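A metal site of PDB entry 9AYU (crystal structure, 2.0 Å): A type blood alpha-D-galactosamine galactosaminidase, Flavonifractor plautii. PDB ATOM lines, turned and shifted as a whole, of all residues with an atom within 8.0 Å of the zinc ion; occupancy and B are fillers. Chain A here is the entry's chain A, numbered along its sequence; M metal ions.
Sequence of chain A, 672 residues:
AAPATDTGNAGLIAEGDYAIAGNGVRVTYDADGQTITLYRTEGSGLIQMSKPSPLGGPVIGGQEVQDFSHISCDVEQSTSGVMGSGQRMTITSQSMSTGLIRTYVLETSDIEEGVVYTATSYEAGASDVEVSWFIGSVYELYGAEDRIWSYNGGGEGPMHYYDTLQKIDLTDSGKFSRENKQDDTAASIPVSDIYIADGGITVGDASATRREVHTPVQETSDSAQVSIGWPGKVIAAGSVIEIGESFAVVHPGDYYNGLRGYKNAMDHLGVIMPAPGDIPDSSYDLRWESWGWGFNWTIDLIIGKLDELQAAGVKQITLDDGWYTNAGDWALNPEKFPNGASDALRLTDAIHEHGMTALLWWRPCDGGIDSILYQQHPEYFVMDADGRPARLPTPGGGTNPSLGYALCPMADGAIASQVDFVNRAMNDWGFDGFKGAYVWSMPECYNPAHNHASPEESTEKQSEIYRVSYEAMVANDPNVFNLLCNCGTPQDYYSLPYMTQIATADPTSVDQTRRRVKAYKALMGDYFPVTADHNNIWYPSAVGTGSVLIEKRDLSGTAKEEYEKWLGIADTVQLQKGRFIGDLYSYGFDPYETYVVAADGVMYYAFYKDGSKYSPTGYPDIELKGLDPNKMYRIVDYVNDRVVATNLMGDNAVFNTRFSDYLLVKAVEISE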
ATOM      1  N   GLU A 379      15.880  12.118  -0.958  1.00  0.00           N
ATOM      2  CA  GLU A 379      15.876  13.487  -1.429  1.00  0.00           C
ATOM      3  C   GLU A 379      17.309  14.031  -1.583  1.00  0.00           C
ATOM      4  O   GLU A 379      17.493  15.010  -2.271  1.00  0.00           O
ATOM      5  CB  GLU A 379      15.010  14.394  -0.529  1.00  0.00           C
ATOM      6  CG  GLU A 379      15.540  14.632   0.884  1.00  0.00           C
ATOM      7  CD  GLU A 379      15.293  13.549   1.935  1.00  0.00           C
ATOM      8  OE1 GLU A 379      15.634  13.809   3.140  1.00  0.00           O
ATOM      9  OE2 GLU A 379      14.762  12.446   1.567  1.00  0.00           O
ATOM     10  N   TYR A 380      18.313  13.377  -0.995  1.00  0.00           N
ATOM     11  CA  TYR A 380      19.699  13.810  -1.151  1.00  0.00           C
ATOM     12  C   TYR A 380      20.313  13.410  -2.488  1.00  0.00           C
ATOM     13  O   TYR A 380      21.415  13.833  -2.782  1.00  0.00           O
ATOM     14  CB  TYR A 380      20.633  13.243  -0.079  1.00  0.00           C
ATOM     15  CG  TYR A 380      20.305  13.596   1.369  1.00  0.00           C
ATOM     16  CD1 TYR A 380      19.388  14.591   1.714  1.00  0.00           C
ATOM     17  CD2 TYR A 380      20.998  12.970   2.400  1.00  0.00           C
ATOM     18  CE1 TYR A 380      19.105  14.865   3.042  1.00  0.00           C
ATOM     19  CE2 TYR A 380      20.739  13.259   3.727  1.00  0.00           C
ATOM     20  CZ  TYR A 380      19.794  14.218   4.048  1.00  0.00           C
ATOM     21  OH  TYR A 380      19.537  14.463   5.352  1.00  0.00           O
ATOM     22  N   PHE A 381      19.603  12.591  -3.284  1.00  0.00           N
ATOM     23  CA  PHE A 381      20.223  11.889  -4.400  1.00  0.00           C
ATOM     24  C   PHE A 381      19.823  12.552  -5.715  1.00  0.00           C
ATOM     25  O   PHE A 381      18.822  13.256  -5.802  1.00  0.00           O
ATOM     26  CB  PHE A 381      19.793  10.424  -4.418  1.00  0.00           C
ATOM     27  CG  PHE A 381      20.416   9.610  -3.296  1.00  0.00           C
ATOM     28  CD1 PHE A 381      21.425   8.686  -3.546  1.00  0.00           C
ATOM     29  CD2 PHE A 381      20.040   9.806  -1.978  1.00  0.00           C
ATOM     30  CE1 PHE A 381      22.001   7.953  -2.528  1.00  0.00           C
ATOM     31  CE2 PHE A 381      20.637   9.093  -0.953  1.00  0.00           C
ATOM     32  CZ  PHE A 381      21.603   8.157  -1.233  1.00  0.00           C
ATOM     33  N   VAL A 382      20.620  12.289  -6.743  1.00  0.00           N
ATOM     34  CA  VAL A 382      20.236  12.698  -8.081  1.00  0.00           C
ATOM     35  C   VAL A 382      19.017  11.899  -8.536  1.00  0.00           C
ATOM     36  O   VAL A 382      18.930  10.685  -8.315  1.00  0.00           O
ATOM     37  CB  VAL A 382      21.409  12.531  -9.071  1.00  0.00           C
ATOM     38  CG1 VAL A 382      20.971  12.891 -10.482  1.00  0.00           C
ATOM     39  CG2 VAL A 382      22.597  13.352  -8.638  1.00  0.00           C
ATOM     40  N   MET A 383      18.105  12.602  -9.182  1.00  0.00           N
ATOM     41  CA  MET A 383      16.902  12.022  -9.748  1.00  0.00           C
ATOM     42  C   MET A 383      16.982  12.177 -11.270  1.00  0.00           C
ATOM     43  O   MET A 383      17.311  13.257 -11.757  1.00  0.00           O
ATOM     44  CB  MET A 383      15.652  12.709  -9.198  1.00  0.00           C
ATOM     45  CG  MET A 383      14.350  12.141  -9.753  1.00  0.00           C
ATOM     46  SD  MET A 383      12.896  12.971  -9.093  1.00  0.00           S
ATOM     47  CE  MET A 383      12.939  12.340  -7.411  1.00  0.00           C
ATOM     48  N   ALA A 406      23.974   8.248  -7.272  1.00  0.00           N
ATOM     49  CA  ALA A 406      24.686   9.498  -7.138  1.00  0.00           C
ATOM     50  C   ALA A 406      24.047  10.426  -6.088  1.00  0.00           C
ATOM     51  O   ALA A 406      22.849  10.652  -6.109  1.00  0.00           O
ATOM     52  CB  ALA A 406      24.736  10.201  -8.492  1.00  0.00           C
ATOM     53  N   LEU A 407      24.883  10.969  -5.214  1.00  0.00           N
ATOM     54  CA  LEU A 407      24.505  12.068  -4.342  1.00  0.00           C
ATOM     55  C   LEU A 407      24.492  13.368  -5.130  1.00  0.00           C
ATOM     56  O   LEU A 407      25.415  13.649  -5.893  1.00  0.00           O
ATOM     57  CB  LEU A 407      25.472  12.170  -3.170  1.00  0.00           C
ATOM     58  CG  LEU A 407      25.404  11.027  -2.162  1.00  0.00           C
ATOM     59  CD1 LEU A 407      26.621  11.101  -1.241  1.00  0.00           C
ATOM     60  CD2 LEU A 407      24.106  11.032  -1.416  1.00  0.00           C
ATOM     61  N   CYS A 408      23.442  14.165  -4.964  1.00  0.00           N
ATOM     62  CA  CYS A 408      23.368  15.433  -5.660  1.00  0.00           C
ATOM     63  C   CYS A 408      24.238  16.469  -4.956  1.00  0.00           C
ATOM     64  O   CYS A 408      24.037  16.711  -3.774  1.00  0.00           O
ATOM     65  CB  CYS A 408      21.951  15.960  -5.790  1.00  0.00           C
ATOM     66  SG  CYS A 408      21.916  17.494  -6.755  1.00  0.00           S
ATOM     67  N   PRO A 409      25.231  17.068  -5.645  1.00  0.00           N
ATOM     68  CA  PRO A 409      26.154  17.977  -4.986  1.00  0.00           C
ATOM     69  C   PRO A 409      25.517  19.256  -4.450  1.00  0.00           C
ATOM     70  O   PRO A 409      26.146  19.949  -3.659  1.00  0.00           O
ATOM     71  CB  PRO A 409      27.216  18.301  -6.047  1.00  0.00           C
ATOM     72  CG  PRO A 409      26.634  17.872  -7.363  1.00  0.00           C
ATOM     73  CD  PRO A 409      25.503  16.898  -7.078  1.00  0.00           C
ATOM     74  N   MET A 410      24.276  19.554  -4.850  1.00  0.00           N
ATOM     75  CA  MET A 410      23.594  20.716  -4.324  1.00  0.00           C
ATOM     76  C   MET A 410      22.641  20.359  -3.189  1.00  0.00           C
ATOM     77  O   MET A 410      21.922  21.234  -2.698  1.00  0.00           O
ATOM     78  CB  MET A 410      22.873  21.448  -5.443  1.00  0.00           C
ATOM     79  CG  MET A 410      23.946  22.188  -6.324  1.00  0.00           C
ATOM     80  SD  MET A 410      22.983  22.973  -7.614  1.00  0.00           S
ATOM     81  CE  MET A 410      22.223  24.311  -6.666  1.00  0.00           C
ATOM     82  N   ALA A 411      22.578  19.091  -2.792  1.00  0.00           N
ATOM     83  CA  ALA A 411      21.740  18.737  -1.648  1.00  0.00           C
ATOM     84  C   ALA A 411      22.594  18.822  -0.385  1.00  0.00           C
ATOM     85  O   ALA A 411      23.623  18.128  -0.282  1.00  0.00           O
ATOM     86  CB  ALA A 411      21.156  17.346  -1.833  1.00  0.00           C
ATOM     87  N   MET A 442      28.974  12.707 -13.078  1.00  0.00           N
ATOM     88  CA  MET A 442      27.848  12.938 -12.190  1.00  0.00           C
ATOM     89  C   MET A 442      26.621  13.117 -13.108  1.00  0.00           C
ATOM     90  O   MET A 442      26.616  13.946 -14.007  1.00  0.00           O
ATOM     91  CB  MET A 442      28.091  14.206 -11.363  1.00  0.00           C
ATOM     92  CG  MET A 442      26.863  14.762 -10.631  1.00  0.00           C
ATOM     93  SD  MET A 442      26.271  13.752  -9.264  1.00  0.00           S
ATOM     94  CE  MET A 442      27.678  13.711  -8.143  1.00  0.00           C
ATOM     95  N   PRO A 443      25.560  12.318 -12.918  1.00  0.00           N
ATOM     96  CA  PRO A 443      24.395  12.429 -13.794  1.00  0.00           C
ATOM     97  C   PRO A 443      23.647  13.745 -13.556  1.00  0.00           C
ATOM     98  O   PRO A 443      23.754  14.354 -12.489  1.00  0.00           O
ATOM     99  CB  PRO A 443      23.566  11.191 -13.465  1.00  0.00           C
ATOM    100  CG  PRO A 443      23.959  10.864 -12.038  1.00  0.00           C
ATOM    101  CD  PRO A 443      25.399  11.310 -11.869  1.00  0.00           C
ATOM    102  N   GLU A 444      22.895  14.121 -14.578  1.00  0.00           N
ATOM    103  CA  GLU A 444      21.988  15.255 -14.526  1.00  0.00           C
ATOM    104  C   GLU A 444      20.859  14.979 -13.557  1.00  0.00           C
ATOM    105  O   GLU A 444      20.380  13.849 -13.463  1.00  0.00           O
ATOM    106  CB  GLU A 444      21.413  15.540 -15.915  1.00  0.00           C
ATOM    107  CG  GLU A 444      22.511  15.929 -16.906  1.00  0.00           C
ATOM    108  CD  GLU A 444      22.046  16.522 -18.215  1.00  0.00           C
ATOM    109  OE1 GLU A 444      22.918  17.171 -18.849  1.00  0.00           O
ATOM    110  OE2 GLU A 444      20.863  16.331 -18.606  1.00  0.00           O
ATOM    111  N   CYS A 445      20.396  16.042 -12.902  1.00  0.00           N
ATOM    112  CA  CYS A 445      19.432  15.923 -11.826  1.00  0.00           C
ATOM    113  C   CYS A 445      18.128  16.655 -12.159  1.00  0.00           C
ATOM    114  O   CYS A 445      18.157  17.835 -12.496  1.00  0.00           O
ATOM    115  CB  CYS A 445      20.003  16.434 -10.510  1.00  0.00           C
ATOM    116  SG  CYS A 445      18.865  16.131  -9.120  1.00  0.00           S
ATOM    117  N   TYR A 446      17.012  15.954 -12.015  1.00  0.00           N
ATOM    118  CA  TYR A 446      15.681  16.467 -12.298  1.00  0.00           C
ATOM    119  C   TYR A 446      14.826  16.544 -11.036  1.00  0.00           C
ATOM    120  O   TYR A 446      13.639  16.722 -11.134  1.00  0.00           O
ATOM    121  CB  TYR A 446      14.955  15.545 -13.289  1.00  0.00           C
ATOM    122  CG  TYR A 446      15.594  15.592 -14.646  1.00  0.00           C
ATOM    123  CD1 TYR A 446      15.047  16.371 -15.668  1.00  0.00           C
ATOM    124  CD2 TYR A 446      16.754  14.893 -14.900  1.00  0.00           C
ATOM    125  CE1 TYR A 446      15.648  16.447 -16.911  1.00  0.00           C
ATOM    126  CE2 TYR A 446      17.371  14.958 -16.132  1.00  0.00           C
ATOM    127  CZ  TYR A 446      16.814  15.741 -17.125  1.00  0.00           C
ATOM    128  OH  TYR A 446      17.417  15.802 -18.323  1.00  0.00           O
ATOM    129  N   ASN A 447      15.406  16.437  -9.858  1.00  0.00           N
ATOM    130  CA  ASN A 447      14.621  16.506  -8.642  1.00  0.00           C
ATOM    131  C   ASN A 447      14.117  17.937  -8.440  1.00  0.00           C
ATOM    132  O   ASN A 447      14.904  18.841  -8.170  1.00  0.00           O
ATOM    133  CB  ASN A 447      15.408  16.021  -7.435  1.00  0.00           C
ATOM    134  CG  ASN A 447      14.510  15.884  -6.225  1.00  0.00           C
ATOM    135  OD1 ASN A 447      13.463  16.525  -6.152  1.00  0.00           O
ATOM    136  ND2 ASN A 447      14.924  15.101  -5.252  1.00  0.00           N
ATOM    137  N   PRO A 448      12.800  18.203  -8.529  1.00  0.00           N
ATOM    138  CA  PRO A 448      12.279  19.576  -8.418  1.00  0.00           C
ATOM    139  C   PRO A 448      12.551  20.181  -7.043  1.00  0.00           C
ATOM    140  O   PRO A 448      12.749  21.397  -6.927  1.00  0.00           O
ATOM    141  CB  PRO A 448      10.787  19.507  -8.769  1.00  0.00           C
ATOM    142  CG  PRO A 448      10.451  18.032  -8.870  1.00  0.00           C
ATOM    143  CD  PRO A 448      11.736  17.211  -8.753  1.00  0.00           C
ATOM    144  N   ALA A 449      12.664  19.347  -6.004  1.00  0.00           N
ATOM    145  CA  ALA A 449      12.971  19.842  -4.676  1.00  0.00           C
ATOM    146  C   ALA A 449      14.362  20.478  -4.599  1.00  0.00           C
ATOM    147  O   ALA A 449      14.669  21.150  -3.612  1.00  0.00           O
ATOM    148  CB  ALA A 449      12.877  18.710  -3.682  1.00  0.00           C
ATOM    149  N   HIS A 450      15.242  20.194  -5.567  1.00  0.00           N
ATOM    150  CA  HIS A 450      16.571  20.781  -5.541  1.00  0.00           C
ATOM    151  C   HIS A 450      16.559  22.150  -6.225  1.00  0.00           C
ATOM    152  O   HIS A 450      17.527  22.891  -6.096  1.00  0.00           O
ATOM    153  CB  HIS A 450      17.630  19.837  -6.164  1.00  0.00           C
ATOM    154  CG  HIS A 450      17.776  18.533  -5.474  1.00  0.00           C
ATOM    155  ND1 HIS A 450      18.509  17.476  -5.983  1.00  0.00           N
ATOM    156  CD2 HIS A 450      17.261  18.093  -4.305  1.00  0.00           C
ATOM    157  CE1 HIS A 450      18.458  16.467  -5.145  1.00  0.00           C
ATOM    158  NE2 HIS A 450      17.693  16.811  -4.116  1.00  0.00           N
ATOM    159  N   ASN A 451      15.503  22.478  -6.995  1.00  0.00           N
ATOM    160  CA  ASN A 451      15.393  23.780  -7.638  1.00  0.00           C
ATOM    161  C   ASN A 451      16.599  24.058  -8.526  1.00  0.00           C
ATOM    162  O   ASN A 451      17.180  25.128  -8.453  1.00  0.00           O
ATOM    163  CB  ASN A 451      15.290  24.941  -6.646  1.00  0.00           C
ATOM    164  CG  ASN A 451      14.017  24.846  -5.828  1.00  0.00           C
ATOM    165  OD1 ASN A 451      12.929  24.999  -6.375  1.00  0.00           O
ATOM    166  ND2 ASN A 451      14.145  24.561  -4.538  1.00  0.00           N
ATOM    167  N   HIS A 452      16.993  23.080  -9.341  1.00  0.00           N
ATOM    168  CA  HIS A 452      18.143  23.278 -10.192  1.00  0.00           C
ATOM    169  C   HIS A 452      17.860  24.323 -11.277  1.00  0.00           C
ATOM    170  O   HIS A 452      16.785  24.390 -11.832  1.00  0.00           O
ATOM    171  CB  HIS A 452      18.551  21.945 -10.827  1.00  0.00           C
ATOM    172  CG  HIS A 452      19.169  20.997  -9.857  1.00  0.00           C
ATOM    173  ND1 HIS A 452      20.396  21.262  -9.269  1.00  0.00           N
ATOM    174  CD2 HIS A 452      18.767  19.792  -9.419  1.00  0.00           C
ATOM    175  CE1 HIS A 452      20.696  20.238  -8.483  1.00  0.00           C
ATOM    176  NE2 HIS A 452      19.747  19.296  -8.593  1.00  0.00           N
ATOM    177  N   SER A 454      19.295  24.209 -14.231  1.00  0.00           N
ATOM    178  CA  SER A 454      19.037  23.282 -15.326  1.00  0.00           C
ATOM    179  C   SER A 454      19.506  21.905 -14.865  1.00  0.00           C
ATOM    180  O   SER A 454      20.193  21.817 -13.851  1.00  0.00           O
ATOM    181  CB  SER A 454      19.759  23.694 -16.571  1.00  0.00           C
ATOM    182  OG  SER A 454      21.168  23.613 -16.283  1.00  0.00           O
ATOM    183  N   PRO A 455      19.161  20.808 -15.556  1.00  0.00           N
ATOM    184  CA  PRO A 455      19.586  19.473 -15.106  1.00  0.00           C
ATOM    185  C   PRO A 455      21.099  19.239 -15.069  1.00  0.00           C
ATOM    186  O   PRO A 455      21.567  18.481 -14.234  1.00  0.00           O
ATOM    187  CB  PRO A 455      18.858  18.527 -16.074  1.00  0.00           C
ATOM    188  CG  PRO A 455      17.695  19.357 -16.604  1.00  0.00           C
ATOM    189  CD  PRO A 455      18.278  20.759 -16.730  1.00  0.00           C
ATOM    190  N   GLU A 457      23.236  21.076 -13.920  1.00  0.00           N
ATOM    191  CA  GLU A 457      23.827  21.744 -12.775  1.00  0.00           C
ATOM    192  C   GLU A 457      24.487  20.742 -11.823  1.00  0.00           C
ATOM    193  O   GLU A 457      25.546  21.020 -11.269  1.00  0.00           O
ATOM    194  CB  GLU A 457      22.732  22.575 -12.126  1.00  0.00           C
ATOM    195  CG  GLU A 457      23.314  23.379 -10.963  1.00  0.00           C
ATOM    196  CD  GLU A 457      22.309  24.317 -10.344  1.00  0.00           C
ATOM    197  OE1 GLU A 457      22.761  25.481 -10.148  1.00  0.00           O
ATOM    198  OE2 GLU A 457      21.125  23.911 -10.143  1.00  0.00           O
ATOM    199  N   SER A 458      23.893  19.561 -11.642  1.00  0.00           N
ATOM    200  CA  SER A 458      24.501  18.542 -10.814  1.00  0.00           C
ATOM    201  C   SER A 458      25.882  18.177 -11.368  1.00  0.00           C
ATOM    202  O   SER A 458      26.864  18.125 -10.614  1.00  0.00           O
ATOM    203  CB  SER A 458      23.604  17.359 -10.688  1.00  0.00           C
ATOM    204  OG  SER A 458      23.140  16.946 -11.966  1.00  0.00           O
ATOM    205  N   THR A 459      25.943  17.912 -12.672  1.00  0.00           N
ATOM    206  CA  THR A 459      27.169  17.534 -13.335  1.00  0.00           C
ATOM    207  C   THR A 459      28.224  18.632 -13.135  1.00  0.00           C
ATOM    208  O   THR A 459      29.366  18.366 -12.806  1.00  0.00           O
ATOM    209  CB  THR A 459      26.907  17.293 -14.831  1.00  0.00           C
ATOM    210  OG1 THR A 459      25.777  16.410 -14.981  1.00  0.00           O
ATOM    211  CG2 THR A 459      28.141  16.767 -15.542  1.00  0.00           C
HETATM  212 ZN    ZN M   1      19.774  17.587  -7.643  1.00  0.00          ZN
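Within 4 Å of the zinc ion: Cys 408, Cys 445, His 450 and His 452.
Along chain A the residues within 4 Å of the zinc ion span positions 408 to 452.
The zinc ion is bound by NE2 of His 452 (2.0 Å), ND1 of His 450 (2.1 Å), SG of Cys 445 (2.3 Å) and SG of Cys 408 (2.3 Å).
N of Cys 445 sits at hydrogen-bond distance from O of Pro 455 (3.0 Å).
The backbone NH (N) of Cys 408 is in hydrogen-bond range of the backbone carbonyl oxygen (O) of Tyr 380, at 3.0 Å.
N of Asn 447 sits close to SG of Cys 445, at 3.6 Å.
SG of Cys 445 lies close to N of Met 383, at 3.6 Å.
ND1 of His 452 is in hydrogen-bond range of OE2 of Glu 457 (2.9 Å).
The side-chain sulfur (SD) of Met 410 is in hydrogen-bond range of a ring nitrogen (ND1) of His 452, 3.5 Å away.
The side-chain amide nitrogen (ND2) of Asn 447 sits at hydrogen-bond distance from a ring nitrogen (NE2) of His 450 (3.4 Å).
N of Cys 445 is in hydrogen-bond range of OG of Ser 458.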
